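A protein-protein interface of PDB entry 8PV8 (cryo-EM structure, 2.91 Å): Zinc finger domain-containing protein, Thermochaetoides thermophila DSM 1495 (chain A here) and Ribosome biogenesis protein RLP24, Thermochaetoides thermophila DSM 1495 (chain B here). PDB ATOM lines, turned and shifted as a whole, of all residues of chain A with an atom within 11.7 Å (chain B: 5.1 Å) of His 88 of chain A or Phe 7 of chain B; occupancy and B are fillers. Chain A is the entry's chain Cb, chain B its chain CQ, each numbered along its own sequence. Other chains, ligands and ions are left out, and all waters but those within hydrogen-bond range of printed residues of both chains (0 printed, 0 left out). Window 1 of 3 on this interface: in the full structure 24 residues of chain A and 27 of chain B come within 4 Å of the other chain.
Printed residues of chain B that touch a printed residue of chain A: Asn 5, Phe 7, Phe 8, Gly 10, Ala 28 and Phe 29.
Hydrophobic or aromatic side chains of chain B that line the printed part of chain A: Phe 7 and Phe 29.
Of the 24 printed residues of chain A, 5 touch a printed residue of chain B.
Hydrophobic or aromatic side chains of chain A that line the printed part of chain B: Tyr 86, His 88, Ala 91 and Ile 95.
Along chain A the printed residues that touch a printed residue of chain B span positions 86 to 95.
Among the printed residues, no Asp or Glu carboxylate lies within 4 Å of a Lys or Arg side-chain nitrogen of the other chain.
Asp 20 of chain A touches none of the printed residues of chain B.
Arg 27 of chain A touches none of the printed residues of chain B.
Of the printed residues of chain B, Tyr 86 of chain A touches Phe 7 and Phe 8.
Printed residues of chain B within 4 Å of Thr 87 of chain A: Phe 7.
His 88 of chain A touches three residues of chain B.
Printed residues of chain B within 4 Å of Ala 91 of chain A: Phe 7.
Of the printed residues of chain A, Asn 5 of chain B touches Ile 95 (3.9 Å).
No residue of chain A comes within 4 Å of Cys 6 of chain B.
Of chain A, only Tyr 86 (2.9 Å), Thr 87 (3.8 Å), His 88 (3.7 Å) and Ala 91 (3.9 Å) come within 4 Å of Phe 7 of chain B.
Of chain A, only Ile 95 (3.4 Å) comes within 4 Å of Gly 10 of chain B.
Ala 28 of chain B touches just one residue of chain A: His 88 (3.0 Å).
Phe 29 of chain B touches one residue of chain A.
Among the printed residues, merely in contact across the chains: Tyr 86 of chain A with Phe 8 of chain B (3.8 Å), Thr 87 of chain A with Phe 7 of chain B (3.8 Å), His 88 of chain A with Phe 7 of chain B (3.7 Å), His 88 of chain A with Phe 29 of chain B (3.4 Å), Ala 91 of chain A with Phe 7 of chain B (3.9 Å), Ile 95 of chain A with Asn 5 of chain B (3.9 Å) and Ile 95 of chain A with Gly 10 of chain B (3.4 Å).
A ring nitrogen (NE2) of His 88 of chain A sits at hydrogen-bond distance from the backbone carbonyl oxygen (O) of Ala 28 of chain B (3.0 Å).
O of Phe 7 of chain B sits at hydrogen-bond distance from OH of Tyr 86 of chain A (2.9 Å).
N of Phe 8 of chain B lies close to SG of Cys 6 of chain B, at 3.3 Å.
OE2 of Glu 89 of chain A is in hydrogen-bond range of OG1 of Thr 87 of chain A (3.2 Å).
The backbone NH of Phe 7 of chain B is in hydrogen-bond range of the backbone carbonyl oxygen of Arg 30 of chain B (2.7 Å).
ND2 of Asn 5 of chain B is in hydrogen-bond range of O of Gly 10 of chain B (3.1 Å).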
ATOM      1  N   ARG A  15     -22.090 -23.054  -7.223  1.00  0.00           N
ATOM      2  CA  ARG A  15     -22.503 -21.673  -7.022  1.00  0.00           C
ATOM      3  C   ARG A  15     -21.652 -20.723  -7.863  1.00  0.00           C
ATOM      4  O   ARG A  15     -20.447 -20.914  -8.043  1.00  0.00           O
ATOM      5  CB  ARG A  15     -22.405 -21.312  -5.540  1.00  0.00           C
ATOM      6  CG  ARG A  15     -22.929 -19.936  -5.185  1.00  0.00           C
ATOM      7  CD  ARG A  15     -22.495 -19.521  -3.795  1.00  0.00           C
ATOM      8  NE  ARG A  15     -22.630 -18.083  -3.602  1.00  0.00           N
ATOM      9  CZ  ARG A  15     -21.704 -17.198  -3.941  1.00  0.00           C
ATOM     10  NH1 ARG A  15     -20.553 -17.572  -4.476  1.00  0.00           N
ATOM     11  NH2 ARG A  15     -21.934 -15.906  -3.733  1.00  0.00           N
ATOM     12  N   ASP A  18     -21.860 -13.530  -7.146  1.00  0.00           N
ATOM     13  CA  ASP A  18     -23.020 -12.670  -6.976  1.00  0.00           C
ATOM     14  C   ASP A  18     -22.828 -11.326  -7.672  1.00  0.00           C
ATOM     15  O   ASP A  18     -21.708 -10.891  -7.966  1.00  0.00           O
ATOM     16  CB  ASP A  18     -23.317 -12.440  -5.493  1.00  0.00           C
ATOM     17  CG  ASP A  18     -23.949 -13.646  -4.831  1.00  0.00           C
ATOM     18  OD1 ASP A  18     -24.931 -14.183  -5.386  1.00  0.00           O
ATOM     19  OD2 ASP A  18     -23.471 -14.055  -3.752  1.00  0.00           O
ATOM     20  N   LEU A  19     -23.960 -10.661  -7.921  1.00  0.00           N
ATOM     21  CA  LEU A  19     -23.941  -9.354  -8.566  1.00  0.00           C
ATOM     22  C   LEU A  19     -23.302  -8.293  -7.683  1.00  0.00           C
ATOM     23  O   LEU A  19     -22.645  -7.385  -8.199  1.00  0.00           O
ATOM     24  CB  LEU A  19     -25.358  -8.933  -8.949  1.00  0.00           C
ATOM     25  CG  LEU A  19     -26.001  -9.726 -10.085  1.00  0.00           C
ATOM     26  CD1 LEU A  19     -27.454  -9.328 -10.268  1.00  0.00           C
ATOM     27  CD2 LEU A  19     -25.226  -9.511 -11.368  1.00  0.00           C
ATOM     28  N   ASP A  20     -23.490  -8.376  -6.364  1.00  0.00           N
ATOM     29  CA  ASP A  20     -22.842  -7.417  -5.475  1.00  0.00           C
ATOM     30  C   ASP A  20     -21.328  -7.598  -5.476  1.00  0.00           C
ATOM     31  O   ASP A  20     -20.578  -6.614  -5.457  1.00  0.00           O
ATOM     32  CB  ASP A  20     -23.429  -7.526  -4.063  1.00  0.00           C
ATOM     33  CG  ASP A  20     -23.323  -8.929  -3.473  1.00  0.00           C
ATOM     34  OD1 ASP A  20     -24.378  -9.508  -3.140  1.00  0.00           O
ATOM     35  OD2 ASP A  20     -22.200  -9.441  -3.296  1.00  0.00           O
ATOM     36  N   GLN A  21     -20.865  -8.851  -5.521  1.00  0.00           N
ATOM     37  CA  GLN A  21     -19.436  -9.117  -5.664  1.00  0.00           C
ATOM     38  C   GLN A  21     -18.907  -8.587  -6.990  1.00  0.00           C
ATOM     39  O   GLN A  21     -17.812  -8.015  -7.040  1.00  0.00           O
ATOM     40  CB  GLN A  21     -19.169 -10.616  -5.544  1.00  0.00           C
ATOM     41  CG  GLN A  21     -19.565 -11.217  -4.213  1.00  0.00           C
ATOM     42  CD  GLN A  21     -19.476 -12.727  -4.214  1.00  0.00           C
ATOM     43  OE1 GLN A  21     -20.147 -13.396  -4.997  1.00  0.00           O
ATOM     44  NE2 GLN A  21     -18.646 -13.273  -3.336  1.00  0.00           N
ATOM     45  N   GLU A  23     -20.162  -6.080  -8.718  1.00  0.00           N
ATOM     46  CA  GLU A  23     -20.159  -4.624  -8.612  1.00  0.00           C
ATOM     47  C   GLU A  23     -18.963  -4.125  -7.808  1.00  0.00           C
ATOM     48  O   GLU A  23     -18.351  -3.106  -8.156  1.00  0.00           O
ATOM     49  CB  GLU A  23     -21.470  -4.154  -7.985  1.00  0.00           C
ATOM     50  CG  GLU A  23     -21.625  -2.650  -7.890  1.00  0.00           C
ATOM     51  CD  GLU A  23     -22.966  -2.244  -7.309  1.00  0.00           C
ATOM     52  OE1 GLU A  23     -23.761  -3.141  -6.963  1.00  0.00           O
ATOM     53  OE2 GLU A  23     -23.225  -1.027  -7.199  1.00  0.00           O
ATOM     54  N   ARG A  24     -18.613  -4.831  -6.728  1.00  0.00           N
ATOM     55  CA  ARG A  24     -17.429  -4.453  -5.961  1.00  0.00           C
ATOM     56  C   ARG A  24     -16.153  -4.672  -6.766  1.00  0.00           C
ATOM     57  O   ARG A  24     -15.190  -3.911  -6.626  1.00  0.00           O
ATOM     58  CB  ARG A  24     -17.375  -5.230  -4.648  1.00  0.00           C
ATOM     59  CG  ARG A  24     -18.489  -4.884  -3.685  1.00  0.00           C
ATOM     60  CD  ARG A  24     -18.418  -5.723  -2.422  1.00  0.00           C
ATOM     61  NE  ARG A  24     -17.210  -5.451  -1.651  1.00  0.00           N
ATOM     62  CZ  ARG A  24     -17.106  -4.499  -0.733  1.00  0.00           C
ATOM     63  NH1 ARG A  24     -18.121  -3.702  -0.444  1.00  0.00           N
ATOM     64  NH2 ARG A  24     -15.952  -4.344  -0.087  1.00  0.00           N
ATOM     65  N   ARG A  27     -16.004  -1.628  -9.109  1.00  0.00           N
ATOM     66  CA  ARG A  27     -15.624  -0.376  -8.461  1.00  0.00           C
ATOM     67  C   ARG A  27     -14.183  -0.409  -7.962  1.00  0.00           C
ATOM     68  O   ARG A  27     -13.453   0.578  -8.105  1.00  0.00           O
ATOM     69  CB  ARG A  27     -16.576  -0.051  -7.311  1.00  0.00           C
ATOM     70  CG  ARG A  27     -17.980   0.296  -7.758  1.00  0.00           C
ATOM     71  CD  ARG A  27     -18.860   0.689  -6.581  1.00  0.00           C
ATOM     72  NE  ARG A  27     -19.162  -0.423  -5.690  1.00  0.00           N
ATOM     73  CZ  ARG A  27     -18.725  -0.520  -4.442  1.00  0.00           C
ATOM     74  NH1 ARG A  27     -17.946   0.407  -3.907  1.00  0.00           N
ATOM     75  NH2 ARG A  27     -19.079  -1.571  -3.709  1.00  0.00           N
ATOM     76  N   GLY A  84     -28.652  -2.123 -10.611  1.00  0.00           N
ATOM     77  CA  GLY A  84     -27.986  -2.170  -9.327  1.00  0.00           C
ATOM     78  C   GLY A  84     -28.228  -3.464  -8.582  1.00  0.00           C
ATOM     79  O   GLY A  84     -29.342  -3.996  -8.593  1.00  0.00           O
ATOM     80  N   ALA A  85     -27.189  -3.983  -7.937  1.00  0.00           N
ATOM     81  CA  ALA A  85     -27.328  -5.203  -7.161  1.00  0.00           C
ATOM     82  C   ALA A  85     -28.065  -4.928  -5.855  1.00  0.00           C
ATOM     83  O   ALA A  85     -28.046  -3.818  -5.316  1.00  0.00           O
ATOM     84  CB  ALA A  85     -25.960  -5.817  -6.871  1.00  0.00           C
ATOM     85  N   TYR A  86     -28.723  -5.963  -5.345  1.00  0.00           N
ATOM     86  CA  TYR A  86     -29.446  -5.877  -4.086  1.00  0.00           C
ATOM     87  C   TYR A  86     -28.482  -6.128  -2.936  1.00  0.00           C
ATOM     88  O   TYR A  86     -27.786  -7.148  -2.914  1.00  0.00           O
ATOM     89  CB  TYR A  86     -30.592  -6.886  -4.061  1.00  0.00           C
ATOM     90  CG  TYR A  86     -31.433  -6.822  -2.814  1.00  0.00           C
ATOM     91  CD1 TYR A  86     -32.390  -5.832  -2.651  1.00  0.00           C
ATOM     92  CD2 TYR A  86     -31.276  -7.757  -1.801  1.00  0.00           C
ATOM     93  CE1 TYR A  86     -33.162  -5.772  -1.514  1.00  0.00           C
ATOM     94  CE2 TYR A  86     -32.046  -7.707  -0.662  1.00  0.00           C
ATOM     95  CZ  TYR A  86     -32.988  -6.712  -0.524  1.00  0.00           C
ATOM     96  OH  TYR A  86     -33.763  -6.652   0.610  1.00  0.00           O
ATOM     97  N   THR A  87     -28.444  -5.201  -1.984  1.00  0.00           N
ATOM     98  CA  THR A  87     -27.463  -5.226  -0.910  1.00  0.00           C
ATOM     99  C   THR A  87     -28.137  -5.091   0.450  1.00  0.00           C
ATOM    100  O   THR A  87     -29.354  -4.895   0.566  1.00  0.00           O
ATOM    101  CB  THR A  87     -26.422  -4.110  -1.085  1.00  0.00           C
ATOM    102  OG1 THR A  87     -27.087  -2.855  -1.275  1.00  0.00           O
ATOM    103  CG2 THR A  87     -25.516  -4.387  -2.276  1.00  0.00           C
ATOM    104  N   HIS A  88     -27.304  -5.198   1.490  1.00  0.00           N
ATOM    105  CA  HIS A  88     -27.780  -5.064   2.862  1.00  0.00           C
ATOM    106  C   HIS A  88     -28.317  -3.670   3.139  1.00  0.00           C
ATOM    107  O   HIS A  88     -29.320  -3.528   3.845  1.00  0.00           O
ATOM    108  CB  HIS A  88     -26.659  -5.397   3.845  1.00  0.00           C
ATOM    109  CG  HIS A  88     -26.365  -6.861   3.955  1.00  0.00           C
ATOM    110  ND1 HIS A  88     -25.381  -7.481   3.217  1.00  0.00           N
ATOM    111  CD2 HIS A  88     -26.923  -7.825   4.724  1.00  0.00           C
ATOM    112  CE1 HIS A  88     -25.348  -8.766   3.523  1.00  0.00           C
ATOM    113  NE2 HIS A  88     -26.274  -9.000   4.435  1.00  0.00           N
ATOM    114  N   GLU A  89     -27.667  -2.637   2.597  1.00  0.00           N
ATOM    115  CA  GLU A  89     -28.139  -1.270   2.793  1.00  0.00           C
ATOM    116  C   GLU A  89     -29.504  -1.066   2.149  1.00  0.00           C
ATOM    117  O   GLU A  89     -30.371  -0.387   2.710  1.00  0.00           O
ATOM    118  CB  GLU A  89     -27.122  -0.277   2.231  1.00  0.00           C
ATOM    119  CG  GLU A  89     -25.737  -0.379   2.850  1.00  0.00           C
ATOM    120  CD  GLU A  89     -24.762  -1.138   1.974  1.00  0.00           C
ATOM    121  OE1 GLU A  89     -23.539  -0.944   2.136  1.00  0.00           O
ATOM    122  OE2 GLU A  89     -25.217  -1.924   1.117  1.00  0.00           O
ATOM    123  N   GLU A  90     -29.717  -1.665   0.976  1.00  0.00           N
ATOM    124  CA  GLU A  90     -31.029  -1.596   0.344  1.00  0.00           C
ATOM    125  C   GLU A  90     -32.068  -2.377   1.142  1.00  0.00           C
ATOM    126  O   GLU A  90     -33.231  -1.967   1.205  1.00  0.00           O
ATOM    127  CB  GLU A  90     -30.951  -2.111  -1.093  1.00  0.00           C
ATOM    128  CG  GLU A  90     -32.256  -1.997  -1.862  1.00  0.00           C
ATOM    129  CD  GLU A  90     -32.131  -2.465  -3.294  1.00  0.00           C
ATOM    130  OE1 GLU A  90     -31.027  -2.901  -3.680  1.00  0.00           O
ATOM    131  OE2 GLU A  90     -33.132  -2.383  -4.035  1.00  0.00           O
ATOM    132  N   ALA A  91     -31.665  -3.487   1.772  1.00  0.00           N
ATOM    133  CA  ALA A  91     -32.588  -4.220   2.639  1.00  0.00           C
ATOM    134  C   ALA A  91     -33.017  -3.381   3.841  1.00  0.00           C
ATOM    135  O   ALA A  91     -34.206  -3.332   4.189  1.00  0.00           O
ATOM    136  CB  ALA A  91     -31.939  -5.523   3.106  1.00  0.00           C
ATOM    137  N   MET A  92     -32.057  -2.708   4.480  1.00  0.00           N
ATOM    138  CA  MET A  92     -32.376  -1.831   5.605  1.00  0.00           C
ATOM    139  C   MET A  92     -33.217  -0.637   5.169  1.00  0.00           C
ATOM    140  O   MET A  92     -34.089  -0.183   5.917  1.00  0.00           O
ATOM    141  CB  MET A  92     -31.093  -1.369   6.290  1.00  0.00           C
ATOM    142  CG  MET A  92     -30.164  -2.498   6.673  1.00  0.00           C
ATOM    143  SD  MET A  92     -29.237  -2.173   8.171  1.00  0.00           S
ATOM    144  CE  MET A  92     -27.895  -1.241   7.447  1.00  0.00           C
ATOM    145  N   ALA A  93     -32.967  -0.110   3.967  1.00  0.00           N
ATOM    146  CA  ALA A  93     -33.795   0.974   3.448  1.00  0.00           C
ATOM    147  C   ALA A  93     -35.215   0.501   3.167  1.00  0.00           C
ATOM    148  O   ALA A  93     -36.179   1.249   3.372  1.00  0.00           O
ATOM    149  CB  ALA A  93     -33.165   1.557   2.183  1.00  0.00           C
ATOM    150  N   ALA A  94     -35.362  -0.733   2.680  1.00  0.00           N
ATOM    151  CA  ALA A  94     -36.687  -1.292   2.436  1.00  0.00           C
ATOM    152  C   ALA A  94     -37.458  -1.483   3.735  1.00  0.00           C
ATOM    153  O   ALA A  94     -38.659  -1.196   3.800  1.00  0.00           O
ATOM    154  CB  ALA A  94     -36.565  -2.616   1.686  1.00  0.00           C
ATOM    155  N   ILE A  95     -36.787  -1.962   4.790  1.00  0.00           N
ATOM    156  CA  ILE A  95     -37.479  -2.189   6.057  1.00  0.00           C
ATOM    157  C   ILE A  95     -37.503  -0.922   6.919  1.00  0.00           C
ATOM    158  O   ILE A  95     -38.146  -0.901   7.978  1.00  0.00           O
ATOM    159  CB  ILE A  95     -36.835  -3.412   6.761  1.00  0.00           C
ATOM    160  CG1 ILE A  95     -37.677  -3.942   7.929  1.00  0.00           C
ATOM    161  CG2 ILE A  95     -35.451  -3.076   7.262  1.00  0.00           C
ATOM    162  CD1 ILE A  95     -39.014  -4.528   7.510  1.00  0.00           C
ATOM    163  N   GLY A  96     -36.892   0.165   6.456  1.00  0.00           N
ATOM    164  CA  GLY A  96     -36.903   1.407   7.217  1.00  0.00           C
ATOM    165  C   GLY A  96     -36.077   1.354   8.482  1.00  0.00           C
ATOM    166  O   GLY A  96     -36.498   1.876   9.522  1.00  0.00           O
ATOM    167  N   TYR A  97     -34.901   0.740   8.413  1.00  0.00           N
ATOM    168  CA  TYR A  97     -34.038   0.521   9.564  1.00  0.00           C
ATOM    169  C   TYR A  97     -32.677   1.134   9.256  1.00  0.00           C
ATOM    170  O   TYR A  97     -32.215   1.072   8.113  1.00  0.00           O
ATOM    171  CB  TYR A  97     -33.930  -0.978   9.849  1.00  0.00           C
ATOM    172  CG  TYR A  97     -33.226  -1.378  11.119  1.00  0.00           C
ATOM    173  CD1 TYR A  97     -33.854  -1.236  12.348  1.00  0.00           C
ATOM    174  CD2 TYR A  97     -31.963  -1.952  11.088  1.00  0.00           C
ATOM    175  CE1 TYR A  97     -33.233  -1.620  13.511  1.00  0.00           C
ATOM    176  CE2 TYR A  97     -31.333  -2.341  12.249  1.00  0.00           C
ATOM    177  CZ  TYR A  97     -31.975  -2.172  13.457  1.00  0.00           C
ATOM    178  OH  TYR A  97     -31.361  -2.558  14.622  1.00  0.00           O
ATOM    179  N   ARG A  98     -32.049   1.744  10.256  1.00  0.00           N
ATOM    180  CA  ARG A  98     -30.843   2.534  10.041  1.00  0.00           C
ATOM    181  C   ARG A  98     -29.798   2.213  11.098  1.00  0.00           C
ATOM    182  O   ARG A  98     -30.132   1.725  12.181  1.00  0.00           O
ATOM    183  CB  ARG A  98     -31.168   4.032  10.047  1.00  0.00           C
ATOM    184  CG  ARG A  98     -32.147   4.459  11.128  1.00  0.00           C
ATOM    185  CD  ARG A  98     -32.271   5.972  11.191  1.00  0.00           C
ATOM    186  NE  ARG A  98     -31.277   6.570  12.073  1.00  0.00           N
ATOM    187  CZ  ARG A  98     -31.431   6.716  13.382  1.00  0.00           C
ATOM    188  NH1 ARG A  98     -32.540   6.336  13.993  1.00  0.00           N
ATOM    189  NH2 ARG A  98     -30.450   7.263  14.094  1.00  0.00           N
ATOM    190  N   ILE A  99     -28.531   2.471  10.769  1.00  0.00           N
ATOM    191  CA  ILE A  99     -27.445   2.271  11.720  1.00  0.00           C
ATOM    192  C   ILE A  99     -27.196   3.560  12.489  1.00  0.00           C
ATOM    193  O   ILE A  99     -27.057   4.641  11.900  1.00  0.00           O
ATOM    194  CB  ILE A  99     -26.170   1.814  10.993  1.00  0.00           C
ATOM    195  CG1 ILE A  99     -26.427   0.540  10.200  1.00  0.00           C
ATOM    196  CG2 ILE A  99     -25.051   1.572  11.981  1.00  0.00           C
ATOM    197  CD1 ILE A  99     -26.858  -0.634  11.036  1.00  0.00           C
ATOM    198  N   ASN B   5     -34.164  -9.373  10.734  1.00  0.00           N
ATOM    199  CA  ASN B   5     -35.017  -9.231   9.565  1.00  0.00           C
ATOM    200  C   ASN B   5     -34.458 -10.080   8.436  1.00  0.00           C
ATOM    201  O   ASN B   5     -33.242 -10.261   8.321  1.00  0.00           O
ATOM    202  CB  ASN B   5     -35.131  -7.773   9.122  1.00  0.00           C
ATOM    203  CG  ASN B   5     -36.197  -7.021   9.884  1.00  0.00           C
ATOM    204  OD1 ASN B   5     -35.902  -6.089  10.631  1.00  0.00           O
ATOM    205  ND2 ASN B   5     -37.448  -7.425   9.704  1.00  0.00           N
ATOM    206  N   CYS B   6     -35.358 -10.617   7.614  1.00  0.00           N
ATOM    207  CA  CYS B   6     -34.939 -11.404   6.464  1.00  0.00           C
ATOM    208  C   CYS B   6     -34.216 -10.521   5.456  1.00  0.00           C
ATOM    209  O   CYS B   6     -34.615  -9.381   5.205  1.00  0.00           O
ATOM    210  CB  CYS B   6     -36.148 -12.072   5.812  1.00  0.00           C
ATOM    211  SG  CYS B   6     -35.773 -13.073   4.355  1.00  0.00           S
ATOM    212  N   PHE B   7     -33.123 -11.045   4.901  1.00  0.00           N
ATOM    213  CA  PHE B   7     -32.385 -10.306   3.883  1.00  0.00           C
ATOM    214  C   PHE B   7     -33.207 -10.143   2.614  1.00  0.00           C
ATOM    215  O   PHE B   7     -33.146  -9.102   1.952  1.00  0.00           O
ATOM    216  CB  PHE B   7     -31.068 -11.016   3.578  1.00  0.00           C
ATOM    217  CG  PHE B   7     -30.299 -10.402   2.450  1.00  0.00           C
ATOM    218  CD1 PHE B   7     -29.651  -9.189   2.612  1.00  0.00           C
ATOM    219  CD2 PHE B   7     -30.225 -11.038   1.223  1.00  0.00           C
ATOM    220  CE1 PHE B   7     -28.944  -8.625   1.571  1.00  0.00           C
ATOM    221  CE2 PHE B   7     -29.522 -10.479   0.179  1.00  0.00           C
ATOM    222  CZ  PHE B   7     -28.878  -9.273   0.354  1.00  0.00           C
ATOM    223  N   PHE B   8     -33.991 -11.159   2.267  1.00  0.00           N
ATOM    224  CA  PHE B   8     -34.670 -11.206   0.981  1.00  0.00           C
ATOM    225  C   PHE B   8     -36.003 -10.468   1.016  1.00  0.00           C
ATOM    226  O   PHE B   8     -36.221  -9.537   0.236  1.00  0.00           O
ATOM    227  CB  PHE B   8     -34.874 -12.661   0.561  1.00  0.00           C
ATOM    228  CG  PHE B   8     -35.027 -12.850  -0.918  1.00  0.00           C
ATOM    229  CD1 PHE B   8     -33.918 -13.049  -1.723  1.00  0.00           C
ATOM    230  CD2 PHE B   8     -36.280 -12.820  -1.504  1.00  0.00           C
ATOM    231  CE1 PHE B   8     -34.058 -13.225  -3.085  1.00  0.00           C
ATOM    232  CE2 PHE B   8     -36.425 -12.989  -2.864  1.00  0.00           C
ATOM    233  CZ  PHE B   8     -35.314 -13.187  -3.656  1.00  0.00           C
ATOM    234  N   CYS B   9     -36.906 -10.874   1.909  1.00  0.00           N
ATOM    235  CA  CYS B   9     -38.238 -10.282   1.915  1.00  0.00           C
ATOM    236  C   CYS B   9     -38.448  -9.303   3.061  1.00  0.00           C
ATOM    237  O   CYS B   9     -39.386  -8.504   3.008  1.00  0.00           O
ATOM    238  CB  CYS B   9     -39.295 -11.376   1.987  1.00  0.00           C
ATOM    239  SG  CYS B   9     -39.397 -12.128   3.608  1.00  0.00           S
ATOM    240  N   GLY B  10     -37.613  -9.347   4.094  1.00  0.00           N
ATOM    241  CA  GLY B  10     -37.731  -8.381   5.167  1.00  0.00           C
ATOM    242  C   GLY B  10     -38.716  -8.739   6.251  1.00  0.00           C
ATOM    243  O   GLY B  10     -39.028  -7.890   7.091  1.00  0.00           O
ATOM    244  N   LYS B  27     -19.473 -11.521   4.543  1.00  0.00           N
ATOM    245  CA  LYS B  27     -20.871 -11.167   4.744  1.00  0.00           C
ATOM    246  C   LYS B  27     -21.702 -12.378   5.146  1.00  0.00           C
ATOM    247  O   LYS B  27     -21.342 -13.527   4.857  1.00  0.00           O
ATOM    248  CB  LYS B  27     -21.463 -10.524   3.487  1.00  0.00           C
ATOM    249  CG  LYS B  27     -20.893  -9.151   3.176  1.00  0.00           C
ATOM    250  CD  LYS B  27     -21.520  -8.553   1.932  1.00  0.00           C
ATOM    251  CE  LYS B  27     -20.930  -7.187   1.619  1.00  0.00           C
ATOM    252  NZ  LYS B  27     -21.491  -6.607   0.367  1.00  0.00           N
ATOM    253  N   ALA B  28     -22.806 -12.106   5.834  1.00  0.00           N
ATOM    254  CA  ALA B  28     -23.776 -13.105   6.244  1.00  0.00           C
ATOM    255  C   ALA B  28     -25.166 -12.676   5.794  1.00  0.00           C
ATOM    256  O   ALA B  28     -25.522 -11.497   5.863  1.00  0.00           O
ATOM    257  CB  ALA B  28     -23.760 -13.301   7.760  1.00  0.00           C
ATOM    258  N   PHE B  29     -25.950 -13.644   5.329  1.00  0.00           N
ATOM    259  CA  PHE B  29     -27.298 -13.389   4.837  1.00  0.00           C
ATOM    260  C   PHE B  29     -28.269 -14.242   5.636  1.00  0.00           C
ATOM    261  O   PHE B  29     -28.143 -15.469   5.657  1.00  0.00           O
ATOM    262  CB  PHE B  29     -27.418 -13.701   3.340  1.00  0.00           C
ATOM    263  CG  PHE B  29     -26.419 -12.975   2.473  1.00  0.00           C
ATOM    264  CD1 PHE B  29     -25.147 -13.485   2.269  1.00  0.00           C
ATOM    265  CD2 PHE B  29     -26.762 -11.786   1.857  1.00  0.00           C
ATOM    266  CE1 PHE B  29     -24.237 -12.820   1.473  1.00  0.00           C
ATOM    267  CE2 PHE B  29     -25.855 -11.116   1.057  1.00  0.00           C
ATOM    268  CZ  PHE B  29     -24.592 -11.634   0.866  1.00  0.00           C
ATOM    269  N   ARG B  30     -29.237 -13.602   6.281  1.00  0.00           N
ATOM    270  CA  ARG B  30     -30.238 -14.298   7.076  1.00  0.00           C
ATOM    271  C   ARG B  30     -31.547 -14.359   6.303  1.00  0.00           C
ATOM    272  O   ARG B  30     -32.073 -13.323   5.883  1.00  0.00           O
ATOM    273  CB  ARG B  30     -30.447 -13.604   8.423  1.00  0.00           C
ATOM    274  CG  ARG B  30     -31.631 -14.127   9.216  1.00  0.00           C
ATOM    275  CD  ARG B  30     -31.374 -15.530   9.737  1.00  0.00           C
ATOM    276  NE  ARG B  30     -32.487 -16.028  10.535  1.00  0.00           N
ATOM    277  CZ  ARG B  30     -32.669 -15.759  11.820  1.00  0.00           C
ATOM    278  NH1 ARG B  30     -31.821 -15.002  12.496  1.00  0.00           N
ATOM    279  NH2 ARG B  30     -33.730 -16.264  12.444  1.00  0.00           N
ATOM    280  N   PHE B  31     -32.064 -15.571   6.114  1.00  0.00           N
ATOM    281  CA  PHE B  31     -33.316 -15.798   5.411  1.00  0.00           C
ATOM    282  C   PHE B  31     -34.330 -16.378   6.381  1.00  0.00           C
ATOM    283  O   PHE B  31     -34.015 -17.291   7.149  1.00  0.00           O
ATOM    284  CB  PHE B  31     -33.123 -16.745   4.230  1.00  0.00           C
ATOM    285  CG  PHE B  31     -32.011 -16.344   3.319  1.00  0.00           C
ATOM    286  CD1 PHE B  31     -32.157 -15.265   2.465  1.00  0.00           C
ATOM    287  CD2 PHE B  31     -30.814 -17.038   3.321  1.00  0.00           C
ATOM    288  CE1 PHE B  31     -31.131 -14.887   1.628  1.00  0.00           C
ATOM    289  CE2 PHE B  31     -29.784 -16.665   2.486  1.00  0.00           C
ATOM    290  CZ  PHE B  31     -29.944 -15.588   1.640  1.00  0.00           C
ATOM    291  N   PHE B  40     -32.928 -16.854  -3.340  1.00  0.00           N
ATOM    292  CA  PHE B  40     -31.564 -16.335  -3.317  1.00  0.00           C
ATOM    293  C   PHE B  40     -30.605 -17.261  -4.060  1.00  0.00           C
ATOM    294  O   PHE B  40     -29.732 -16.800  -4.803  1.00  0.00           O
ATOM    295  CB  PHE B  40     -31.107 -16.136  -1.873  1.00  0.00           C
ATOM    296  CG  PHE B  40     -29.722 -15.569  -1.746  1.00  0.00           C
ATOM    297  CD1 PHE B  40     -29.502 -14.209  -1.897  1.00  0.00           C
ATOM    298  CD2 PHE B  40     -28.640 -16.391  -1.468  1.00  0.00           C
ATOM    299  CE1 PHE B  40     -28.230 -13.682  -1.777  1.00  0.00           C
ATOM    300  CE2 PHE B  40     -27.368 -15.870  -1.349  1.00  0.00           C
ATOM    301  CZ  PHE B  40     -27.163 -14.513  -1.504  1.00  0.00           C
